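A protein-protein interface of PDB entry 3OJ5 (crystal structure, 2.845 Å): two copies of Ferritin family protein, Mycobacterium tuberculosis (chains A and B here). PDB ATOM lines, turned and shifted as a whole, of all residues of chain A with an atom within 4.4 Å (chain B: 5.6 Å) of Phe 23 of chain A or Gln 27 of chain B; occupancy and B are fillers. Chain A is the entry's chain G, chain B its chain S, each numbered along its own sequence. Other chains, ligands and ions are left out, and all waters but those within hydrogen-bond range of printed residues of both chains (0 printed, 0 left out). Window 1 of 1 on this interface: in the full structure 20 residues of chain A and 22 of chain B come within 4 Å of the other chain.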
ATOM      1  N   ILE A  19     -22.751  -3.509  16.243  1.00  0.00           N
ATOM      2  CA  ILE A  19     -22.563  -4.611  15.323  1.00  0.00           C
ATOM      3  C   ILE A  19     -22.964  -4.179  13.917  1.00  0.00           C
ATOM      4  O   ILE A  19     -22.208  -4.387  12.959  1.00  0.00           O
ATOM      5  CB  ILE A  19     -23.347  -5.840  15.781  1.00  0.00           C
ATOM      6  CG1 ILE A  19     -22.714  -6.379  17.082  1.00  0.00           C
ATOM      7  CG2 ILE A  19     -23.368  -6.884  14.664  1.00  0.00           C
ATOM      8  CD1 ILE A  19     -23.456  -7.539  17.691  1.00  0.00           C
ATOM      9  N   HIS A  20     -24.136  -3.546  13.797  1.00  0.00           N
ATOM     10  CA  HIS A  20     -24.602  -2.986  12.520  1.00  0.00           C
ATOM     11  C   HIS A  20     -23.600  -1.956  11.972  1.00  0.00           C
ATOM     12  O   HIS A  20     -23.245  -1.967  10.780  1.00  0.00           O
ATOM     13  CB  HIS A  20     -25.972  -2.350  12.709  1.00  0.00           C
ATOM     14  CG  HIS A  20     -26.546  -1.784  11.452  1.00  0.00           C
ATOM     15  ND1 HIS A  20     -27.072  -2.576  10.462  1.00  0.00           N
ATOM     16  CD2 HIS A  20     -26.631  -0.503  11.023  1.00  0.00           C
ATOM     17  CE1 HIS A  20     -27.493  -1.800   9.468  1.00  0.00           C
ATOM     18  NE2 HIS A  20     -27.221  -0.547   9.775  1.00  0.00           N
ATOM     19  N   ASN A  21     -23.127  -1.074  12.849  1.00  0.00           N
ATOM     20  CA  ASN A  21     -22.148  -0.061  12.451  1.00  0.00           C
ATOM     21  C   ASN A  21     -20.835  -0.663  11.911  1.00  0.00           C
ATOM     22  O   ASN A  21     -20.369  -0.269  10.836  1.00  0.00           O
ATOM     23  CB  ASN A  21     -21.861   0.922  13.601  1.00  0.00           C
ATOM     24  CG  ASN A  21     -23.083   1.748  13.998  1.00  0.00           C
ATOM     25  OD1 ASN A  21     -24.063   1.881  13.235  1.00  0.00           O
ATOM     26  ND2 ASN A  21     -23.039   2.293  15.211  1.00  0.00           N
ATOM     27  N   GLU A  22     -20.251  -1.619  12.636  1.00  0.00           N
ATOM     28  CA  GLU A  22     -18.992  -2.199  12.194  1.00  0.00           C
ATOM     29  C   GLU A  22     -19.186  -2.987  10.906  1.00  0.00           C
ATOM     30  O   GLU A  22     -18.320  -2.984  10.041  1.00  0.00           O
ATOM     31  CB  GLU A  22     -18.300  -3.043  13.267  1.00  0.00           C
ATOM     32  CG  GLU A  22     -18.213  -2.377  14.627  1.00  0.00           C
ATOM     33  CD  GLU A  22     -16.965  -1.503  14.832  1.00  0.00           C
ATOM     34  OE1 GLU A  22     -16.183  -1.335  13.855  1.00  0.00           O
ATOM     35  OE2 GLU A  22     -16.773  -0.987  15.983  1.00  0.00           O
ATOM     36  N   PHE A  23     -20.324  -3.665  10.748  1.00  0.00           N
ATOM     37  CA  PHE A  23     -20.532  -4.423   9.499  1.00  0.00           C
ATOM     38  C   PHE A  23     -20.600  -3.450   8.339  1.00  0.00           C
ATOM     39  O   PHE A  23     -20.105  -3.758   7.253  1.00  0.00           O
ATOM     40  CB  PHE A  23     -21.773  -5.297   9.557  1.00  0.00           C
ATOM     41  CG  PHE A  23     -21.507  -6.693  10.040  1.00  0.00           C
ATOM     42  CD1 PHE A  23     -20.613  -7.514   9.377  1.00  0.00           C
ATOM     43  CD2 PHE A  23     -22.187  -7.208  11.124  1.00  0.00           C
ATOM     44  CE1 PHE A  23     -20.373  -8.808   9.793  1.00  0.00           C
ATOM     45  CE2 PHE A  23     -21.964  -8.503  11.546  1.00  0.00           C
ATOM     46  CZ  PHE A  23     -21.030  -9.299  10.891  1.00  0.00           C
ATOM     47  N   THR A  24     -21.209  -2.283   8.583  1.00  0.00           N
ATOM     48  CA  THR A  24     -21.261  -1.252   7.568  1.00  0.00           C
ATOM     49  C   THR A  24     -19.881  -0.628   7.304  1.00  0.00           C
ATOM     50  O   THR A  24     -19.483  -0.477   6.149  1.00  0.00           O
ATOM     51  CB  THR A  24     -22.279  -0.203   7.925  1.00  0.00           C
ATOM     52  OG1 THR A  24     -23.582  -0.819   7.920  1.00  0.00           O
ATOM     53  CG2 THR A  24     -22.201   0.938   6.912  1.00  0.00           C
ATOM     54  N   ALA A  25     -19.176  -0.248   8.372  1.00  0.00           N
ATOM     55  CA  ALA A  25     -17.820   0.279   8.261  1.00  0.00           C
ATOM     56  C   ALA A  25     -16.965  -0.645   7.374  1.00  0.00           C
ATOM     57  O   ALA A  25     -16.323  -0.204   6.395  1.00  0.00           O
ATOM     58  CB  ALA A  25     -17.209   0.416   9.630  1.00  0.00           C
ATOM     59  N   ALA A  26     -17.004  -1.931   7.691  1.00  0.00           N
ATOM     60  CA  ALA A  26     -16.277  -2.921   6.918  1.00  0.00           C
ATOM     61  C   ALA A  26     -16.644  -2.862   5.433  1.00  0.00           C
ATOM     62  O   ALA A  26     -15.755  -2.826   4.553  1.00  0.00           O
ATOM     63  CB  ALA A  26     -16.510  -4.317   7.492  1.00  0.00           C
ATOM     64  N   GLN A  27     -17.945  -2.810   5.158  1.00  0.00           N
ATOM     65  CA  GLN A  27     -18.424  -2.757   3.781  1.00  0.00           C
ATOM     66  C   GLN A  27     -17.924  -1.481   3.059  1.00  0.00           C
ATOM     67  O   GLN A  27     -17.585  -1.506   1.862  1.00  0.00           O
ATOM     68  CB  GLN A  27     -19.961  -2.872   3.746  1.00  0.00           C
ATOM     69  CG  GLN A  27     -20.531  -3.244   2.390  1.00  0.00           C
ATOM     70  CD  GLN A  27     -20.136  -4.650   1.934  1.00  0.00           C
ATOM     71  OE1 GLN A  27     -19.233  -5.284   2.498  1.00  0.00           O
ATOM     72  NE2 GLN A  27     -20.824  -5.149   0.910  1.00  0.00           N
ATOM     73  N   ALA A  59     -16.537  -6.554  14.385  1.00  0.00           N
ATOM     74  CA  ALA A  59     -17.969  -6.853  14.403  1.00  0.00           C
ATOM     75  C   ALA A  59     -18.196  -8.170  15.134  1.00  0.00           C
ATOM     76  O   ALA A  59     -19.050  -8.294  16.016  1.00  0.00           O
ATOM     77  CB  ALA A  59     -18.546  -6.904  12.975  1.00  0.00           C
ATOM     78  N   MET A  60     -17.370  -9.149  14.788  1.00  0.00           N
ATOM     79  CA  MET A  60     -17.487 -10.489  15.347  1.00  0.00           C
ATOM     80  C   MET A  60     -16.979 -10.586  16.797  1.00  0.00           C
ATOM     81  O   MET A  60     -17.477 -11.423  17.548  1.00  0.00           O
ATOM     82  CB  MET A  60     -16.835 -11.485  14.406  1.00  0.00           C
ATOM     83  CG  MET A  60     -17.368 -11.420  12.989  1.00  0.00           C
ATOM     84  SD  MET A  60     -18.841 -12.436  12.746  1.00  0.00           S
ATOM     85  CE  MET A  60     -20.036 -11.474  13.686  1.00  0.00           C
ATOM     86  N   ILE A  75     -27.396 -10.925  13.433  1.00  0.00           N
ATOM     87  CA  ILE A  75     -26.535 -10.500  12.356  1.00  0.00           C
ATOM     88  C   ILE A  75     -27.406  -9.605  11.488  1.00  0.00           C
ATOM     89  O   ILE A  75     -28.415 -10.065  10.966  1.00  0.00           O
ATOM     90  CB  ILE A  75     -25.976 -11.713  11.560  1.00  0.00           C
ATOM     91  CG1 ILE A  75     -25.006 -12.509  12.444  1.00  0.00           C
ATOM     92  CG2 ILE A  75     -25.269 -11.275  10.280  1.00  0.00           C
ATOM     93  CD1 ILE A  75     -23.940 -11.663  13.121  1.00  0.00           C
ATOM     94  N   PRO A  76     -27.025  -8.314  11.342  1.00  0.00           N
ATOM     95  CA  PRO A  76     -27.863  -7.329  10.628  1.00  0.00           C
ATOM     96  C   PRO A  76     -27.555  -7.301   9.146  1.00  0.00           C
ATOM     97  O   PRO A  76     -26.564  -7.923   8.699  1.00  0.00           O
ATOM     98  CB  PRO A  76     -27.428  -5.991  11.242  1.00  0.00           C
ATOM     99  CG  PRO A  76     -25.922  -6.186  11.476  1.00  0.00           C
ATOM    100  CD  PRO A  76     -25.781  -7.697  11.862  1.00  0.00           C
ATOM    101  N   VAL A  78     -26.694  -4.546   5.880  1.00  0.00           N
ATOM    102  CA  VAL A  78     -25.722  -3.459   5.814  1.00  0.00           C
ATOM    103  C   VAL A  78     -26.242  -2.323   4.961  1.00  0.00           C
ATOM    104  O   VAL A  78     -26.745  -2.571   3.862  1.00  0.00           O
ATOM    105  CB  VAL A  78     -24.369  -3.955   5.259  1.00  0.00           C
ATOM    106  CG1 VAL A  78     -23.389  -2.791   5.145  1.00  0.00           C
ATOM    107  CG2 VAL A  78     -23.800  -5.088   6.160  1.00  0.00           C
ATOM    108  N   GLU B  22     -24.381 -12.416  -3.512  1.00  0.00           N
ATOM    109  CA  GLU B  22     -23.376 -13.185  -2.764  1.00  0.00           C
ATOM    110  C   GLU B  22     -23.014 -12.504  -1.445  1.00  0.00           C
ATOM    111  O   GLU B  22     -22.754 -13.196  -0.451  1.00  0.00           O
ATOM    112  CB  GLU B  22     -22.113 -13.510  -3.581  1.00  0.00           C
ATOM    113  CG  GLU B  22     -22.376 -14.089  -4.970  1.00  0.00           C
ATOM    114  CD  GLU B  22     -22.457 -15.608  -5.020  1.00  0.00           C
ATOM    115  OE1 GLU B  22     -22.381 -16.251  -3.934  1.00  0.00           O
ATOM    116  OE2 GLU B  22     -22.582 -16.149  -6.166  1.00  0.00           O
ATOM    117  N   PHE B  23     -22.998 -11.168  -1.416  1.00  0.00           N
ATOM    118  CA  PHE B  23     -22.706 -10.485  -0.140  1.00  0.00           C
ATOM    119  C   PHE B  23     -23.790 -10.813   0.863  1.00  0.00           C
ATOM    120  O   PHE B  23     -23.489 -11.013   2.048  1.00  0.00           O
ATOM    121  CB  PHE B  23     -22.556  -8.966  -0.293  1.00  0.00           C
ATOM    122  CG  PHE B  23     -21.166  -8.541  -0.588  1.00  0.00           C
ATOM    123  CD1 PHE B  23     -20.154  -8.813   0.321  1.00  0.00           C
ATOM    124  CD2 PHE B  23     -20.849  -7.902  -1.780  1.00  0.00           C
ATOM    125  CE1 PHE B  23     -18.833  -8.456   0.064  1.00  0.00           C
ATOM    126  CE2 PHE B  23     -19.536  -7.537  -2.051  1.00  0.00           C
ATOM    127  CZ  PHE B  23     -18.518  -7.836  -1.123  1.00  0.00           C
ATOM    128  N   THR B  24     -25.039 -10.890   0.369  1.00  0.00           N
ATOM    129  CA  THR B  24     -26.189 -11.287   1.191  1.00  0.00           C
ATOM    130  C   THR B  24     -26.105 -12.743   1.655  1.00  0.00           C
ATOM    131  O   THR B  24     -26.237 -13.035   2.840  1.00  0.00           O
ATOM    132  CB  THR B  24     -27.512 -11.043   0.478  1.00  0.00           C
ATOM    133  OG1 THR B  24     -27.647  -9.632   0.251  1.00  0.00           O
ATOM    134  CG2 THR B  24     -28.651 -11.508   1.374  1.00  0.00           C
ATOM    135  N   ALA B  25     -25.899 -13.658   0.706  1.00  0.00           N
ATOM    136  CA  ALA B  25     -25.630 -15.075   1.023  1.00  0.00           C
ATOM    137  C   ALA B  25     -24.602 -15.180   2.148  1.00  0.00           C
ATOM    138  O   ALA B  25     -24.840 -15.801   3.180  1.00  0.00           O
ATOM    139  CB  ALA B  25     -25.154 -15.815  -0.204  1.00  0.00           C
ATOM    140  N   ALA B  26     -23.478 -14.523   1.964  1.00  0.00           N
ATOM    141  CA  ALA B  26     -22.435 -14.550   2.960  1.00  0.00           C
ATOM    142  C   ALA B  26     -22.991 -14.160   4.319  1.00  0.00           C
ATOM    143  O   ALA B  26     -22.732 -14.846   5.329  1.00  0.00           O
ATOM    144  CB  ALA B  26     -21.269 -13.625   2.528  1.00  0.00           C
ATOM    145  N   GLN B  27     -23.744 -13.065   4.343  1.00  0.00           N
ATOM    146  CA  GLN B  27     -24.247 -12.523   5.604  1.00  0.00           C
ATOM    147  C   GLN B  27     -25.222 -13.504   6.248  1.00  0.00           C
ATOM    148  O   GLN B  27     -25.223 -13.663   7.474  1.00  0.00           O
ATOM    149  CB  GLN B  27     -24.880 -11.139   5.397  1.00  0.00           C
ATOM    150  CG  GLN B  27     -25.083 -10.353   6.675  1.00  0.00           C
ATOM    151  CD  GLN B  27     -23.767  -9.892   7.327  1.00  0.00           C
ATOM    152  OE1 GLN B  27     -22.690 -10.374   6.988  1.00  0.00           O
ATOM    153  NE2 GLN B  27     -23.860  -8.953   8.269  1.00  0.00           N
ATOM    154  N   GLN B  28     -26.024 -14.169   5.407  1.00  0.00           N
ATOM    155  CA  GLN B  28     -26.960 -15.175   5.858  1.00  0.00           C
ATOM    156  C   GLN B  28     -26.248 -16.349   6.547  1.00  0.00           C
ATOM    157  O   GLN B  28     -26.698 -16.823   7.611  1.00  0.00           O
ATOM    158  CB  GLN B  28     -27.835 -15.679   4.703  1.00  0.00           C
ATOM    159  CG  GLN B  28     -28.935 -16.674   5.168  1.00  0.00           C
ATOM    160  CD  GLN B  28     -29.866 -16.079   6.237  1.00  0.00           C
ATOM    161  OE1 GLN B  28     -30.839 -15.370   5.913  1.00  0.00           O
ATOM    162  NE2 GLN B  28     -29.559 -16.342   7.513  1.00  0.00           N
ATOM    163  N   TYR B  29     -25.152 -16.822   5.935  1.00  0.00           N
ATOM    164  CA  TYR B  29     -24.295 -17.825   6.570  1.00  0.00           C
ATOM    165  C   TYR B  29     -23.740 -17.410   7.927  1.00  0.00           C
ATOM    166  O   TYR B  29     -23.772 -18.202   8.852  1.00  0.00           O
ATOM    167  CB  TYR B  29     -23.178 -18.274   5.655  1.00  0.00           C
ATOM    168  CG  TYR B  29     -23.697 -19.165   4.564  1.00  0.00           C
ATOM    169  CD1 TYR B  29     -24.881 -19.854   4.736  1.00  0.00           C
ATOM    170  CD2 TYR B  29     -23.012 -19.308   3.353  1.00  0.00           C
ATOM    171  CE1 TYR B  29     -25.380 -20.679   3.744  1.00  0.00           C
ATOM    172  CE2 TYR B  29     -23.500 -20.139   2.344  1.00  0.00           C
ATOM    173  CZ  TYR B  29     -24.689 -20.826   2.546  1.00  0.00           C
ATOM    174  OH  TYR B  29     -25.183 -21.648   1.546  1.00  0.00           O
ATOM    175  N   VAL B  30     -23.223 -16.197   8.064  1.00  0.00           N
ATOM    176  CA  VAL B  30     -22.808 -15.734   9.390  1.00  0.00           C
ATOM    177  C   VAL B  30     -23.953 -15.857  10.396  1.00  0.00           C
ATOM    178  O   VAL B  30     -23.787 -16.422  11.496  1.00  0.00           O
ATOM    179  CB  VAL B  30     -22.289 -14.289   9.368  1.00  0.00           C
ATOM    180  CG1 VAL B  30     -21.943 -13.812  10.786  1.00  0.00           C
ATOM    181  CG2 VAL B  30     -21.093 -14.195   8.442  1.00  0.00           C
ATOM    182  N   ALA B  31     -25.127 -15.351  10.006  1.00  0.00           N
ATOM    183  CA  ALA B  31     -26.320 -15.458  10.865  1.00  0.00           C
ATOM    184  C   ALA B  31     -26.538 -16.912  11.303  1.00  0.00           C
ATOM    185  O   ALA B  31     -26.676 -17.194  12.500  1.00  0.00           O
ATOM    186  CB  ALA B  31     -27.556 -14.909  10.168  1.00  0.00           C
ATOM    187  N   ILE B  32     -26.541 -17.824  10.330  1.00  0.00           N
ATOM    188  CA  ILE B  32     -26.726 -19.237  10.610  1.00  0.00           C
ATOM    189  C   ILE B  32     -25.641 -19.718  11.564  1.00  0.00           C
ATOM    190  O   ILE B  32     -25.975 -20.366  12.559  1.00  0.00           O
ATOM    191  CB  ILE B  32     -26.812 -20.085   9.304  1.00  0.00           C
ATOM    192  CG1 ILE B  32     -28.168 -19.844   8.624  1.00  0.00           C
ATOM    193  CG2 ILE B  32     -26.644 -21.539   9.594  1.00  0.00           C
ATOM    194  CD1 ILE B  32     -28.289 -20.481   7.256  1.00  0.00           C
ATOM    195  N   VAL B  78     -26.357  -4.719   2.153  1.00  0.00           N
ATOM    196  CA  VAL B  78     -26.799  -6.103   2.315  1.00  0.00           C
ATOM    197  C   VAL B  78     -28.196  -6.175   2.944  1.00  0.00           C
ATOM    198  O   VAL B  78     -28.443  -5.547   3.976  1.00  0.00           O
ATOM    199  CB  VAL B  78     -25.817  -6.929   3.172  1.00  0.00           C
ATOM    200  CG1 VAL B  78     -26.329  -8.372   3.304  1.00  0.00           C
ATOM    201  CG2 VAL B  78     -24.402  -6.871   2.573  1.00  0.00           C
ATOM    202  N   ASP B  79     -29.099  -6.935   2.326  1.00  0.00           N
ATOM    203  CA  ASP B  79     -30.444  -7.092   2.846  1.00  0.00           C
ATOM    204  C   ASP B  79     -30.431  -7.715   4.251  1.00  0.00           C
ATOM    205  O   ASP B  79     -29.499  -8.445   4.611  1.00  0.00           O
ATOM    206  CB  ASP B  79     -31.222  -7.987   1.899  1.00  0.00           C
ATOM    207  CG  ASP B  79     -31.767  -7.234   0.724  1.00  0.00           C
ATOM    208  OD1 ASP B  79     -32.080  -6.051   0.918  1.00  0.00           O
ATOM    209  OD2 ASP B  79     -31.807  -7.805  -0.387  1.00  0.00           O
ATOM    210  N   VAL B  81     -31.078 -10.394   7.049  1.00  0.00           N
ATOM    211  CA  VAL B  81     -31.004 -11.856   6.868  1.00  0.00           C
ATOM    212  C   VAL B  81     -31.733 -12.547   8.005  1.00  0.00           C
ATOM    213  O   VAL B  81     -32.001 -11.939   9.071  1.00  0.00           O
ATOM    214  CB  VAL B  81     -29.533 -12.375   6.755  1.00  0.00           C
ATOM    215  CG1 VAL B  81     -28.897 -11.856   5.448  1.00  0.00           C
ATOM    216  CG2 VAL B  81     -28.694 -11.977   8.004  1.00  0.00           C
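The side-chain amide nitrogen of Gln 27 of chain B is in hydrogen-bond range of the backbone carbonyl oxygen of Pro 76 of chain A (2.9 Å). O of Val 78 of chain A lies within hydrogen-bond range of N of Val 78 of chain B, at 2.8 Å.
Among the printed residues, merely in contact across the chains: Ile 75 of chain A with Gln 27 of chain B, Ile 75 of chain A with Val 81 of chain B, Ile 75 of chain A with Ala 31 of chain B, Phe 23 of chain A with Gln 27 of chain B, Ile 75 of chain A with Val 30 of chain B, Gln 27 of chain A with Phe 23 of chain B and Met 60 of chain A with Val 30 of chain B.
Of chain A, only Phe 23, Ile 75 and Pro 76 come within 4 Å of Gln 27 of chain B. Of the printed residues of chain B, Gln 27 of chain A touches Phe 23 (3.7 Å). Of the printed residues of chain A, Ala 31 of chain B touches Ile 75 (3.6 Å). Printed residues of chain A within 4 Å of Val 81 of chain B: Ile 75 (3.5 Å). Of the printed residues of chain B, Met 60 of chain A touches Val 30. The nearest residue of chain B that does not touch Phe 23 of chain A is Val 30 of chain B (4.6 Å). The nearest printed residue of chain A that does not touch Gln 27 of chain B is Val 78 of chain A (4.4 Å). The nearest printed residue of chain A that does not touch Phe 23 of chain B is Val 78 of chain A (7.2 Å).
Hydrophobic or aromatic side chains of chain B that line the printed part of chain A: Phe 23, Val 30, Ala 31, Val 78 and Val 81. Hydrophobic or aromatic side chains of chain A within 4 Å of the printed part of chain B: Phe 23, Met 60, Ile 75 and Val 78. Among the printed residues, 9 pairs touch across the chains.
Phe 23 of chain A touches Gln 27 of chain B, and with the chains exchanged Gln 27 of chain A touches Phe 23 of chain B. Val 78 of chain A touches its own counterpart, Val 78 of chain B. Positions printed for both chains: 22, 23, 24, 25, 26, 27 and 78. Of the 9 pairs that touch across the chains among the printed residues, 3 have their exchanged pair printed and touching as well.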
